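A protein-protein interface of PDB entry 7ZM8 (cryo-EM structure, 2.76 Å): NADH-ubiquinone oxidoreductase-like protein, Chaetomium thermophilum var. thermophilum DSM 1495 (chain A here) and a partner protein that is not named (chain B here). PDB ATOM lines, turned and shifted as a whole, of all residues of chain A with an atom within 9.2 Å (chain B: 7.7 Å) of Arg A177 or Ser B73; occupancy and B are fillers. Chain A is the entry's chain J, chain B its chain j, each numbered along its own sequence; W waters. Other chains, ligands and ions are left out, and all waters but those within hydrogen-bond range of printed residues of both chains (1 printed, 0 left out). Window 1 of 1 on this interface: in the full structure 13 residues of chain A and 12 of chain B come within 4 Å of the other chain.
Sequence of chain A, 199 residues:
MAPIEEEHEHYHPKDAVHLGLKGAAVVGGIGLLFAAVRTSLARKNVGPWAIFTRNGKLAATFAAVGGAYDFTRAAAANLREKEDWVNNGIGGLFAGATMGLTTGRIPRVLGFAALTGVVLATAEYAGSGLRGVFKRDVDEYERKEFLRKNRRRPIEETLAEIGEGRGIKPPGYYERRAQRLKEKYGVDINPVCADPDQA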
ATOM      1  N   GLU A 164       4.378  28.662  35.906  1.00  0.00           N
ATOM      2  CA  GLU A 164       3.103  29.168  35.343  1.00  0.00           C
ATOM      3  C   GLU A 164       2.046  28.068  35.425  1.00  0.00           C
ATOM      4  O   GLU A 164       2.424  26.890  35.389  1.00  0.00           O
ATOM      5  CB  GLU A 164       3.297  29.674  33.920  1.00  0.00           C
ATOM      6  CG  GLU A 164       4.519  30.554  33.770  1.00  0.00           C
ATOM      7  CD  GLU A 164       4.784  31.015  32.350  1.00  0.00           C
ATOM      8  OE1 GLU A 164       5.826  31.663  32.131  1.00  0.00           O
ATOM      9  OE2 GLU A 164       3.947  30.725  31.472  1.00  0.00           O
ATOM     10  N   GLY A 165       0.772  28.444  35.525  1.00  0.00           N
ATOM     11  CA  GLY A 165      -0.309  27.468  35.705  1.00  0.00           C
ATOM     12  C   GLY A 165      -0.817  27.538  37.121  1.00  0.00           C
ATOM     13  O   GLY A 165      -0.221  28.278  37.901  1.00  0.00           O
ATOM     14  N   LYS A 169      -1.187  32.825  35.558  1.00  0.00           N
ATOM     15  CA  LYS A 169      -1.155  32.964  34.083  1.00  0.00           C
ATOM     16  C   LYS A 169      -0.464  34.287  33.772  1.00  0.00           C
ATOM     17  O   LYS A 169      -1.138  35.319  33.723  1.00  0.00           O
ATOM     18  CB  LYS A 169      -2.566  32.761  33.530  1.00  0.00           C
ATOM     19  CG  LYS A 169      -3.116  31.359  33.756  1.00  0.00           C
ATOM     20  CD  LYS A 169      -4.602  31.316  34.005  1.00  0.00           C
ATOM     21  CE  LYS A 169      -5.424  31.507  32.750  1.00  0.00           C
ATOM     22  NZ  LYS A 169      -5.330  30.333  31.853  1.00  0.00           N
ATOM     23  N   PRO A 170       0.864  34.279  33.543  1.00  0.00           N
ATOM     24  CA  PRO A 170       1.614  35.507  33.317  1.00  0.00           C
ATOM     25  C   PRO A 170       1.294  36.054  31.920  1.00  0.00           C
ATOM     26  O   PRO A 170       0.845  35.275  31.115  1.00  0.00           O
ATOM     27  CB  PRO A 170       3.073  35.068  33.503  1.00  0.00           C
ATOM     28  CG  PRO A 170       2.970  33.729  34.178  1.00  0.00           C
ATOM     29  CD  PRO A 170       1.739  33.115  33.555  1.00  0.00           C
ATOM     30  N   GLY A 172       1.134  36.378  28.261  1.00  0.00           N
ATOM     31  CA  GLY A 172       1.766  35.512  27.244  1.00  0.00           C
ATOM     32  C   GLY A 172       1.573  34.032  27.529  1.00  0.00           C
ATOM     33  O   GLY A 172       2.202  33.228  26.838  1.00  0.00           O
ATOM     34  N   TYR A 173       0.729  33.688  28.502  1.00  0.00           N
ATOM     35  CA  TYR A 173       0.519  32.276  28.910  1.00  0.00           C
ATOM     36  C   TYR A 173      -0.159  31.490  27.785  1.00  0.00           C
ATOM     37  O   TYR A 173       0.213  30.328  27.580  1.00  0.00           O
ATOM     38  CB  TYR A 173      -0.270  32.208  30.222  1.00  0.00           C
ATOM     39  CG  TYR A 173      -0.722  30.833  30.638  1.00  0.00           C
ATOM     40  CD1 TYR A 173       0.102  30.003  31.376  1.00  0.00           C
ATOM     41  CD2 TYR A 173      -1.981  30.362  30.303  1.00  0.00           C
ATOM     42  CE1 TYR A 173      -0.304  28.736  31.753  1.00  0.00           C
ATOM     43  CE2 TYR A 173      -2.403  29.098  30.673  1.00  0.00           C
ATOM     44  CZ  TYR A 173      -1.561  28.282  31.403  1.00  0.00           C
ATOM     45  OH  TYR A 173      -1.967  27.037  31.778  1.00  0.00           O
ATOM     46  N   TYR A 174      -1.141  32.083  27.113  1.00  0.00           N
ATOM     47  CA  TYR A 174      -1.922  31.351  26.084  1.00  0.00           C
ATOM     48  C   TYR A 174      -1.068  30.970  24.868  1.00  0.00           C
ATOM     49  O   TYR A 174      -1.199  29.836  24.383  1.00  0.00           O
ATOM     50  CB  TYR A 174      -3.187  32.132  25.730  1.00  0.00           C
ATOM     51  CG  TYR A 174      -4.194  32.241  26.844  1.00  0.00           C
ATOM     52  CD1 TYR A 174      -4.602  31.122  27.550  1.00  0.00           C
ATOM     53  CD2 TYR A 174      -4.750  33.459  27.186  1.00  0.00           C
ATOM     54  CE1 TYR A 174      -5.530  31.213  28.574  1.00  0.00           C
ATOM     55  CE2 TYR A 174      -5.684  33.566  28.202  1.00  0.00           C
ATOM     56  CZ  TYR A 174      -6.072  32.441  28.903  1.00  0.00           C
ATOM     57  OH  TYR A 174      -6.989  32.545  29.907  1.00  0.00           O
ATOM     58  N   GLU A 175      -0.241  31.891  24.378  1.00  0.00           N
ATOM     59  CA  GLU A 175       0.639  31.607  23.214  1.00  0.00           C
ATOM     60  C   GLU A 175       1.652  30.527  23.587  1.00  0.00           C
ATOM     61  O   GLU A 175       1.943  29.678  22.744  1.00  0.00           O
ATOM     62  CB  GLU A 175       1.351  32.884  22.769  1.00  0.00           C
ATOM     63  N   ARG A 176       2.200  30.602  24.792  1.00  0.00           N
ATOM     64  CA  ARG A 176       3.154  29.567  25.250  1.00  0.00           C
ATOM     65  C   ARG A 176       2.426  28.230  25.377  1.00  0.00           C
ATOM     66  O   ARG A 176       3.016  27.207  25.038  1.00  0.00           O
ATOM     67  CB  ARG A 176       3.858  30.001  26.538  1.00  0.00           C
ATOM     68  CG  ARG A 176       4.779  31.202  26.386  1.00  0.00           C
ATOM     69  CD  ARG A 176       5.554  31.517  27.655  1.00  0.00           C
ATOM     70  NE  ARG A 176       4.729  31.902  28.794  1.00  0.00           N
ATOM     71  CZ  ARG A 176       4.441  33.153  29.131  1.00  0.00           C
ATOM     72  NH1 ARG A 176       3.679  33.398  30.182  1.00  0.00           N
ATOM     73  NH2 ARG A 176       4.913  34.158  28.416  1.00  0.00           N
ATOM     74  N   ARG A 177       1.191  28.251  25.869  1.00  0.00           N
ATOM     75  CA  ARG A 177       0.450  26.995  26.120  1.00  0.00           C
ATOM     76  C   ARG A 177       0.171  26.370  24.774  1.00  0.00           C
ATOM     77  O   ARG A 177       0.268  25.147  24.668  1.00  0.00           O
ATOM     78  CB  ARG A 177      -0.844  27.263  26.891  1.00  0.00           C
ATOM     79  CG  ARG A 177      -1.523  26.017  27.437  1.00  0.00           C
ATOM     80  CD  ARG A 177      -2.869  26.327  28.053  1.00  0.00           C
ATOM     81  NE  ARG A 177      -3.924  26.130  27.076  1.00  0.00           N
ATOM     82  CZ  ARG A 177      -4.847  25.183  27.159  1.00  0.00           C
ATOM     83  NH1 ARG A 177      -5.765  25.070  26.220  1.00  0.00           N
ATOM     84  NH2 ARG A 177      -4.861  24.364  28.190  1.00  0.00           N
ATOM     85  N   ALA A 178      -0.150  27.197  23.789  1.00  0.00           N
ATOM     86  CA  ALA A 178      -0.335  26.652  22.450  1.00  0.00           C
ATOM     87  C   ALA A 178       0.919  25.935  21.981  1.00  0.00           C
ATOM     88  O   ALA A 178       0.854  24.815  21.463  1.00  0.00           O
ATOM     89  CB  ALA A 178      -0.706  27.770  21.481  1.00  0.00           C
ATOM     90  N   GLN A 179       2.078  26.568  22.162  1.00  0.00           N
ATOM     91  CA  GLN A 179       3.331  25.935  21.778  1.00  0.00           C
ATOM     92  C   GLN A 179       3.579  24.674  22.591  1.00  0.00           C
ATOM     93  O   GLN A 179       4.037  23.660  22.057  1.00  0.00           O
ATOM     94  CB  GLN A 179       4.482  26.924  21.948  1.00  0.00           C
ATOM     95  CG  GLN A 179       5.826  26.384  21.501  1.00  0.00           C
ATOM     96  CD  GLN A 179       5.878  26.141  20.009  1.00  0.00           C
ATOM     97  OE1 GLN A 179       5.377  26.942  19.222  1.00  0.00           O
ATOM     98  NE2 GLN A 179       6.482  25.028  19.612  1.00  0.00           N
ATOM     99  N   ARG A 180       3.293  24.725  23.891  1.00  0.00           N
ATOM    100  CA  ARG A 180       3.474  23.551  24.737  1.00  0.00           C
ATOM    101  C   ARG A 180       2.539  22.423  24.319  1.00  0.00           C
ATOM    102  O   ARG A 180       2.959  21.269  24.194  1.00  0.00           O
ATOM    103  CB  ARG A 180       3.244  23.936  26.195  1.00  0.00           C
ATOM    104  CG  ARG A 180       3.496  22.835  27.187  1.00  0.00           C
ATOM    105  CD  ARG A 180       3.593  23.394  28.596  1.00  0.00           C
ATOM    106  NE  ARG A 180       2.386  24.115  28.993  1.00  0.00           N
ATOM    107  CZ  ARG A 180       2.285  25.439  29.023  1.00  0.00           C
ATOM    108  NH1 ARG A 180       1.154  26.013  29.396  1.00  0.00           N
ATOM    109  NH2 ARG A 180       3.320  26.186  28.676  1.00  0.00           N
ATOM    110  N   LEU A 181       1.264  22.745  24.093  1.00  0.00           N
ATOM    111  CA  LEU A 181       0.291  21.722  23.734  1.00  0.00           C
ATOM    112  C   LEU A 181       0.564  21.145  22.357  1.00  0.00           C
ATOM    113  O   LEU A 181       0.358  19.948  22.138  1.00  0.00           O
ATOM    114  CB  LEU A 181      -1.121  22.301  23.791  1.00  0.00           C
ATOM    115  CG  LEU A 181      -1.958  22.058  25.047  1.00  0.00           C
ATOM    116  CD1 LEU A 181      -1.265  22.600  26.280  1.00  0.00           C
ATOM    117  CD2 LEU A 181      -3.321  22.695  24.880  1.00  0.00           C
ATOM    118  N   LYS A 182       1.012  21.979  21.417  1.00  0.00           N
ATOM    119  CA  LYS A 182       1.341  21.487  20.084  1.00  0.00           C
ATOM    120  C   LYS A 182       2.495  20.496  20.132  1.00  0.00           C
ATOM    121  O   LYS A 182       2.473  19.470  19.444  1.00  0.00           O
ATOM    122  CB  LYS A 182       1.682  22.659  19.167  1.00  0.00           C
ATOM    123  CG  LYS A 182       2.251  22.252  17.820  1.00  0.00           C
ATOM    124  CD  LYS A 182       1.213  21.542  16.971  1.00  0.00           C
ATOM    125  CE  LYS A 182       1.789  21.137  15.626  1.00  0.00           C
ATOM    126  NZ  LYS A 182       2.159  22.324  14.808  1.00  0.00           N
ATOM    127  N   GLU A 183       3.514  20.786  20.941  1.00  0.00           N
ATOM    128  CA  GLU A 183       4.676  19.909  21.011  1.00  0.00           C
ATOM    129  C   GLU A 183       4.313  18.548  21.591  1.00  0.00           C
ATOM    130  O   GLU A 183       4.797  17.513  21.120  1.00  0.00           O
ATOM    131  CB  GLU A 183       5.779  20.570  21.836  1.00  0.00           C
ATOM    132  CG  GLU A 183       7.096  19.813  21.833  1.00  0.00           C
ATOM    133  CD  GLU A 183       8.202  20.570  22.541  1.00  0.00           C
ATOM    134  OE1 GLU A 183       7.929  21.670  23.065  1.00  0.00           O
ATOM    135  OE2 GLU A 183       9.345  20.069  22.571  1.00  0.00           O
ATOM    136  N   LYS A 184       3.459  18.527  22.613  1.00  0.00           N
ATOM    137  CA  LYS A 184       3.174  17.301  23.347  1.00  0.00           C
ATOM    138  C   LYS A 184       1.991  16.522  22.800  1.00  0.00           C
ATOM    139  O   LYS A 184       2.023  15.288  22.807  1.00  0.00           O
ATOM    140  CB  LYS A 184       2.920  17.615  24.825  1.00  0.00           C
ATOM    141  CG  LYS A 184       2.753  16.379  25.695  1.00  0.00           C
ATOM    142  CD  LYS A 184       2.515  16.742  27.146  1.00  0.00           C
ATOM    143  CE  LYS A 184       3.780  17.299  27.779  1.00  0.00           C
ATOM    144  NZ  LYS A 184       4.843  16.263  27.891  1.00  0.00           N
ATOM    145  N   TYR A 185       0.984  17.229  22.313  1.00  0.00           N
ATOM    146  CA  TYR A 185      -0.262  16.573  21.844  1.00  0.00           C
ATOM    147  C   TYR A 185      -0.315  16.489  20.316  1.00  0.00           C
ATOM    148  O   TYR A 185      -1.092  15.673  19.787  1.00  0.00           O
ATOM    149  CB  TYR A 185      -1.495  17.163  22.531  1.00  0.00           C
ATOM    150  CG  TYR A 185      -1.531  16.952  24.021  1.00  0.00           C
ATOM    151  CD1 TYR A 185      -1.859  15.720  24.559  1.00  0.00           C
ATOM    152  CD2 TYR A 185      -1.232  17.981  24.896  1.00  0.00           C
ATOM    153  CE1 TYR A 185      -1.894  15.516  25.928  1.00  0.00           C
ATOM    154  CE2 TYR A 185      -1.259  17.794  26.267  1.00  0.00           C
ATOM    155  CZ  TYR A 185      -1.591  16.556  26.784  1.00  0.00           C
ATOM    156  OH  TYR A 185      -1.623  16.363  28.135  1.00  0.00           O
ATOM    157  N   VAL A 187      -1.528  18.752  18.266  1.00  0.00           N
ATOM    158  CA  VAL A 187      -2.791  19.309  17.797  1.00  0.00           C
ATOM    159  C   VAL A 187      -2.731  20.819  17.958  1.00  0.00           C
ATOM    160  O   VAL A 187      -2.322  21.319  19.013  1.00  0.00           O
ATOM    161  CB  VAL A 187      -3.995  18.731  18.565  1.00  0.00           C
ATOM    162  CG1 VAL A 187      -5.279  19.411  18.122  1.00  0.00           C
ATOM    163  CG2 VAL A 187      -4.091  17.228  18.355  1.00  0.00           C
ATOM    164  N   ASP A 188      -3.133  21.542  16.918  1.00  0.00           N
ATOM    165  CA  ASP A 188      -3.159  22.995  16.962  1.00  0.00           C
ATOM    166  C   ASP A 188      -4.445  23.471  17.623  1.00  0.00           C
ATOM    167  O   ASP A 188      -5.535  22.983  17.309  1.00  0.00           O
ATOM    168  CB  ASP A 188      -3.042  23.579  15.554  1.00  0.00           C
ATOM    169  N   ILE A 189      -4.314  24.423  18.540  1.00  0.00           N
ATOM    170  CA  ILE A 189      -5.465  24.964  19.255  1.00  0.00           C
ATOM    171  C   ILE A 189      -6.091  26.068  18.413  1.00  0.00           C
ATOM    172  O   ILE A 189      -5.406  27.003  17.986  1.00  0.00           O
ATOM    173  CB  ILE A 189      -5.062  25.487  20.640  1.00  0.00           C
ATOM    174  CG1 ILE A 189      -4.708  24.328  21.570  1.00  0.00           C
ATOM    175  CG2 ILE A 189      -6.173  26.337  21.232  1.00  0.00           C
ATOM    176  CD1 ILE A 189      -5.786  23.277  21.683  1.00  0.00           C
ATOM    177  N   ASN A 190      -7.398  25.966  18.177  1.00  0.00           N
ATOM    178  CA  ASN A 190      -8.126  26.949  17.375  1.00  0.00           C
ATOM    179  C   ASN A 190      -9.565  26.966  17.857  1.00  0.00           C
ATOM    180  O   ASN A 190     -10.432  26.281  17.302  1.00  0.00           O
ATOM    181  CB  ASN A 190      -8.056  26.624  15.885  1.00  0.00           C
ATOM    182  CG  ASN A 190      -8.618  27.730  15.015  1.00  0.00           C
ATOM    183  OD1 ASN A 190      -9.095  28.750  15.511  1.00  0.00           O
ATOM    184  ND2 ASN A 190      -8.569  27.527  13.703  1.00  0.00           N
ATOM    185  N   PRO A 191      -9.857  27.734  18.903  1.00  0.00           N
ATOM    186  CA  PRO A 191     -11.212  27.736  19.464  1.00  0.00           C
ATOM    187  C   PRO A 191     -12.248  28.279  18.487  1.00  0.00           C
ATOM    188  O   PRO A 191     -11.946  29.095  17.615  1.00  0.00           O
ATOM    189  CB  PRO A 191     -11.070  28.635  20.692  1.00  0.00           C
ATOM    190  CG  PRO A 191      -9.650  28.498  21.080  1.00  0.00           C
ATOM    191  CD  PRO A 191      -8.902  28.413  19.789  1.00  0.00           C
ATOM    192  N   GLY B  59      -2.645  21.025  38.508  1.00  0.00           N
ATOM    193  CA  GLY B  59      -2.552  21.983  37.388  1.00  0.00           C
ATOM    194  C   GLY B  59      -2.660  21.306  36.034  1.00  0.00           C
ATOM    195  O   GLY B  59      -2.345  21.954  35.033  1.00  0.00           O
ATOM    196  N   LEU B  60      -3.002  20.022  36.010  1.00  0.00           N
ATOM    197  CA  LEU B  60      -3.126  19.269  34.735  1.00  0.00           C
ATOM    198  C   LEU B  60      -4.316  19.760  33.907  1.00  0.00           C
ATOM    199  O   LEU B  60      -4.186  19.810  32.681  1.00  0.00           O
ATOM    200  CB  LEU B  60      -3.229  17.771  35.027  1.00  0.00           C
ATOM    201  CG  LEU B  60      -3.004  16.843  33.836  1.00  0.00           C
ATOM    202  CD1 LEU B  60      -1.786  17.272  33.034  1.00  0.00           C
ATOM    203  CD2 LEU B  60      -2.853  15.404  34.299  1.00  0.00           C
ATOM    204  N   TRP B  61      -5.440  20.085  34.542  1.00  0.00           N
ATOM    205  CA  TRP B  61      -6.649  20.427  33.753  1.00  0.00           C
ATOM    206  C   TRP B  61      -7.289  21.747  34.174  1.00  0.00           C
ATOM    207  O   TRP B  61      -7.155  22.108  35.356  1.00  0.00           O
ATOM    208  CB  TRP B  61      -7.686  19.303  33.874  1.00  0.00           C
ATOM    209  CG  TRP B  61      -7.221  17.952  33.435  1.00  0.00           C
ATOM    210  CD1 TRP B  61      -6.901  17.556  32.170  1.00  0.00           C
ATOM    211  CD2 TRP B  61      -7.062  16.794  34.271  1.00  0.00           C
ATOM    212  NE1 TRP B  61      -6.538  16.236  32.164  1.00  0.00           N
ATOM    213  CE2 TRP B  61      -6.629  15.743  33.439  1.00  0.00           C
ATOM    214  CE3 TRP B  61      -7.233  16.550  35.637  1.00  0.00           C
ATOM    215  CZ2 TRP B  61      -6.370  14.467  33.931  1.00  0.00           C
ATOM    216  CZ3 TRP B  61      -6.978  15.288  36.123  1.00  0.00           C
ATOM    217  CH2 TRP B  61      -6.550  14.264  35.280  1.00  0.00           C
ATOM    218  N   ASP B  62      -7.948  22.433  33.237  1.00  0.00           N
ATOM    219  CA  ASP B  62      -8.727  23.653  33.543  1.00  0.00           C
ATOM    220  C   ASP B  62      -9.932  23.622  32.619  1.00  0.00           C
ATOM    221  O   ASP B  62      -9.755  23.334  31.439  1.00  0.00           O
ATOM    222  CB  ASP B  62      -7.954  24.952  33.373  1.00  0.00           C
ATOM    223  CG  ASP B  62      -8.787  26.196  33.609  1.00  0.00           C
ATOM    224  OD1 ASP B  62      -9.416  26.282  34.677  1.00  0.00           O
ATOM    225  OD2 ASP B  62      -8.805  27.064  32.714  1.00  0.00           O
ATOM    226  N   LEU B  63     -11.126  23.934  33.119  1.00  0.00           N
ATOM    227  CA  LEU B  63     -12.352  23.833  32.287  1.00  0.00           C
ATOM    228  C   LEU B  63     -12.890  25.218  31.926  1.00  0.00           C
ATOM    229  O   LEU B  63     -13.730  25.277  31.024  1.00  0.00           O
ATOM    230  CB  LEU B  63     -13.424  23.088  33.089  1.00  0.00           C
ATOM    231  CG  LEU B  63     -13.215  21.604  33.370  1.00  0.00           C
ATOM    232  CD1 LEU B  63     -14.510  20.989  33.875  1.00  0.00           C
ATOM    233  CD2 LEU B  63     -12.764  20.876  32.123  1.00  0.00           C
ATOM    234  N   LYS B  66     -13.074  26.980  28.207  1.00  0.00           N
ATOM    235  CA  LYS B  66     -12.575  26.055  27.199  1.00  0.00           C
ATOM    236  C   LYS B  66     -13.706  25.641  26.274  1.00  0.00           C
ATOM    237  O   LYS B  66     -14.733  25.133  26.727  1.00  0.00           O
ATOM    238  CB  LYS B  66     -11.980  24.820  27.860  1.00  0.00           C
ATOM    239  CG  LYS B  66     -10.837  25.099  28.791  1.00  0.00           C
ATOM    240  CD  LYS B  66      -9.524  25.160  28.062  1.00  0.00           C
ATOM    241  CE  LYS B  66      -8.412  25.494  29.023  1.00  0.00           C
ATOM    242  NZ  LYS B  66      -7.839  24.271  29.631  1.00  0.00           N
ATOM    243  N   GLY B  69     -12.147  22.951  19.941  1.00  0.00           N
ATOM    244  CA  GLY B  69     -10.896  23.379  19.367  1.00  0.00           C
ATOM    245  C   GLY B  69      -9.811  23.655  20.379  1.00  0.00           C
ATOM    246  O   GLY B  69      -8.638  23.727  20.000  1.00  0.00           O
ATOM    247  N   ASP B  70     -10.169  23.828  21.645  1.00  0.00           N
ATOM    248  CA  ASP B  70      -9.242  23.956  22.755  1.00  0.00           C
ATOM    249  C   ASP B  70      -9.128  22.613  23.462  1.00  0.00           C
ATOM    250  O   ASP B  70      -9.955  21.718  23.277  1.00  0.00           O
ATOM    251  CB  ASP B  70      -9.716  25.036  23.735  1.00  0.00           C
ATOM    252  CG  ASP B  70      -8.575  25.753  24.426  1.00  0.00           C
ATOM    253  OD1 ASP B  70      -7.412  25.331  24.274  1.00  0.00           O
ATOM    254  OD2 ASP B  70      -8.844  26.753  25.123  1.00  0.00           O
ATOM    255  N   LEU B  71      -8.062  22.437  24.235  1.00  0.00           N
ATOM    256  CA  LEU B  71      -7.848  21.175  24.978  1.00  0.00           C
ATOM    257  C   LEU B  71      -8.002  21.465  26.469  1.00  0.00           C
ATOM    258  O   LEU B  71      -7.629  22.559  26.894  1.00  0.00           O
ATOM    259  CB  LEU B  71      -6.465  20.605  24.639  1.00  0.00           C
ATOM    260  CG  LEU B  71      -6.318  19.943  23.271  1.00  0.00           C
ATOM    261  CD1 LEU B  71      -4.941  19.323  23.130  1.00  0.00           C
ATOM    262  CD2 LEU B  71      -7.392  18.892  23.053  1.00  0.00           C
ATOM    263  N   ILE B  72      -8.606  20.552  27.213  1.00  0.00           N
ATOM    264  CA  ILE B  72      -8.780  20.716  28.688  1.00  0.00           C
ATOM    265  C   ILE B  72      -7.399  20.753  29.344  1.00  0.00           C
ATOM    266  O   ILE B  72      -7.224  21.527  30.294  1.00  0.00           O
ATOM    267  CB  ILE B  72      -9.673  19.595  29.273  1.00  0.00           C
ATOM    268  CG1 ILE B  72     -10.986  19.444  28.503  1.00  0.00           C
ATOM    269  CG2 ILE B  72      -9.910  19.794  30.757  1.00  0.00           C
ATOM    270  CD1 ILE B  72     -11.848  18.309  28.988  1.00  0.00           C
ATOM    271  N   SER B  73      -6.458  19.960  28.846  1.00  0.00           N
ATOM    272  CA  SER B  73      -5.113  19.847  29.469  1.00  0.00           C
ATOM    273  C   SER B  73      -4.318  21.156  29.462  1.00  0.00           C
ATOM    274  O   SER B  73      -4.069  21.678  28.367  1.00  0.00           O
ATOM    275  CB  SER B  73      -4.347  18.749  28.815  1.00  0.00           C
ATOM    276  OG  SER B  73      -4.835  17.483  29.221  1.00  0.00           O
ATOM    277  N   GLU B  74      -3.958  21.673  30.638  1.00  0.00           N
ATOM    278  CA  GLU B  74      -3.101  22.846  30.727  1.00  0.00           C
ATOM    279  C   GLU B  74      -1.672  22.529  30.328  1.00  0.00           C
ATOM    280  O   GLU B  74      -1.011  23.346  29.680  1.00  0.00           O
ATOM    281  CB  GLU B  74      -3.091  23.399  32.151  1.00  0.00           C
ATOM    282  CG  GLU B  74      -4.422  23.820  32.726  1.00  0.00           C
ATOM    283  CD  GLU B  74      -4.263  24.371  34.132  1.00  0.00           C
ATOM    284  OE1 GLU B  74      -3.108  24.606  34.550  1.00  0.00           O
ATOM    285  OE2 GLU B  74      -5.278  24.568  34.827  1.00  0.00           O
ATOM    286  N   ARG B  75      -1.184  21.358  30.715  1.00  0.00           N
ATOM    287  CA  ARG B  75       0.230  21.035  30.661  1.00  0.00           C
ATOM    288  C   ARG B  75       0.498  19.952  29.625  1.00  0.00           C
ATOM    289  O   ARG B  75       1.552  19.921  28.989  1.00  0.00           O
ATOM    290  CB  ARG B  75       0.701  20.600  32.051  1.00  0.00           C
ATOM    291  CG  ARG B  75       1.972  19.780  32.097  1.00  0.00           C
ATOM    292  CD  ARG B  75       2.507  19.717  33.519  1.00  0.00           C
ATOM    293  NE  ARG B  75       1.760  18.783  34.360  1.00  0.00           N
ATOM    294  CZ  ARG B  75       0.894  19.146  35.301  1.00  0.00           C
ATOM    295  NH1 ARG B  75       0.274  18.226  36.020  1.00  0.00           N
ATOM    296  NH2 ARG B  75       0.648  20.426  35.521  1.00  0.00           N
ATOM    297  OXT ARG B  75      -0.347  19.088  29.389  1.00  0.00           O
HETATM  298  O   HOH W   1      -3.740  27.440  34.146  1.00  0.00           O
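The guanidinium group (NH1) of Arg A177 is in salt-bridge range of the side-chain carboxylate (OD1) of Asp B70, 2.6 Å away.
NH1 of Arg A180 sits at hydrogen-bond distance from O of Glu B74.
The backbone carbonyl oxygen of Leu B71 sits at hydrogen-bond distance from the guanidinium group of Arg A177.
The backbone NH of Asn A190 lies within hydrogen-bond range of the backbone carbonyl oxygen of Gly B69, 3.1 Å away.
The backbone carbonyl oxygen (O) of Ser B73 sits at hydrogen-bond distance from the guanidinium group (NH2) of Arg A177, at 2.8 Å.
The side-chain hydroxyl (OH) of Tyr A185 is in hydrogen-bond range of the chain-end carboxylate (OXT) of Arg B75 (3.3 Å).
The side-chain amino group (NZ) of Lys B66 sits close to the guanidinium group (NH2) of Arg A177.
N of Glu B74 is in hydrogen-bond range of O of Leu B60 (2.8 Å).
O of Ile B72 lies within hydrogen-bond range of NZ of Lys B66 (2.9 Å).
The guanidinium group (NH2) of Arg B75 sits at hydrogen-bond distance from the backbone carbonyl oxygen (O) of Gly B59, at 3.4 Å.
The backbone carbonyl oxygen (O) of Leu B71 is in hydrogen-bond range of the side-chain amino group (NZ) of Lys B66 (3.2 Å).
The backbone carbonyl oxygen (O) of Asp B62 lies within hydrogen-bond range of the side-chain amino group (NZ) of Lys B66, at 2.8 Å.
Among the printed residues, merely in contact across the chains: Ile A189 with Gly B69 (3.3 Å), Ile A189 with Asp B70 (3.4 Å), Arg A177 with Glu B74 (3.4 Å), Leu A181 with Glu B74 (3.5 Å), Ile A189 with Leu B71 (3.5 Å), Tyr A185 with Ser B73 (3.6 Å), Leu A181 with Ser B73 (3.6 Å), Lys A184 with Arg B75 (3.6 Å), Leu A181 with Leu B71 (3.8 Å), Tyr A173 with Glu B74 (3.8 Å) and Arg A180 with Arg B75 (3.9 Å).
Arg A177 touches just these residues of chain B: Lys B66, Asp B70, Leu B71, Ser B73 and Glu B74.
Of chain A, only Arg A177, Leu A181 and Tyr A185 come within 4 Å of Ser B73.
Printed residues of chain B within 4 Å of Tyr A185: Ser B73 (3.6 Å) and Arg B75 (3.3 Å).
Printed residues of chain A within 4 Å of Glu B74: Tyr A173, Arg A177, Arg A180 and Leu A181.
Tyr A174 touches none of the printed residues of chain B.
Of the 13 printed residues of chain B, 7 touch a printed residue of chain A.
Printed residues of chain B that touch a printed residue of chain A: Lys B66, Gly B69, Asp B70, Leu B71, Ser B73, Glu B74 and Arg B75.
Hydrophobic or aromatic side chains of chain B that line the printed part of chain A: Leu B71.
Hydrophobic or aromatic side chains of chain A within 4 Å of the printed part of chain B: Tyr A173, Leu A181, Tyr A185 and Ile A189.
Among the printed residues, 18 pairs touch across the chains.
Water W1 bridges the side-chain carboxylate (OE1) of Glu B74 (2.9 Å) and the side-chain hydroxyl (OH) of Tyr A173 (3.0 Å).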
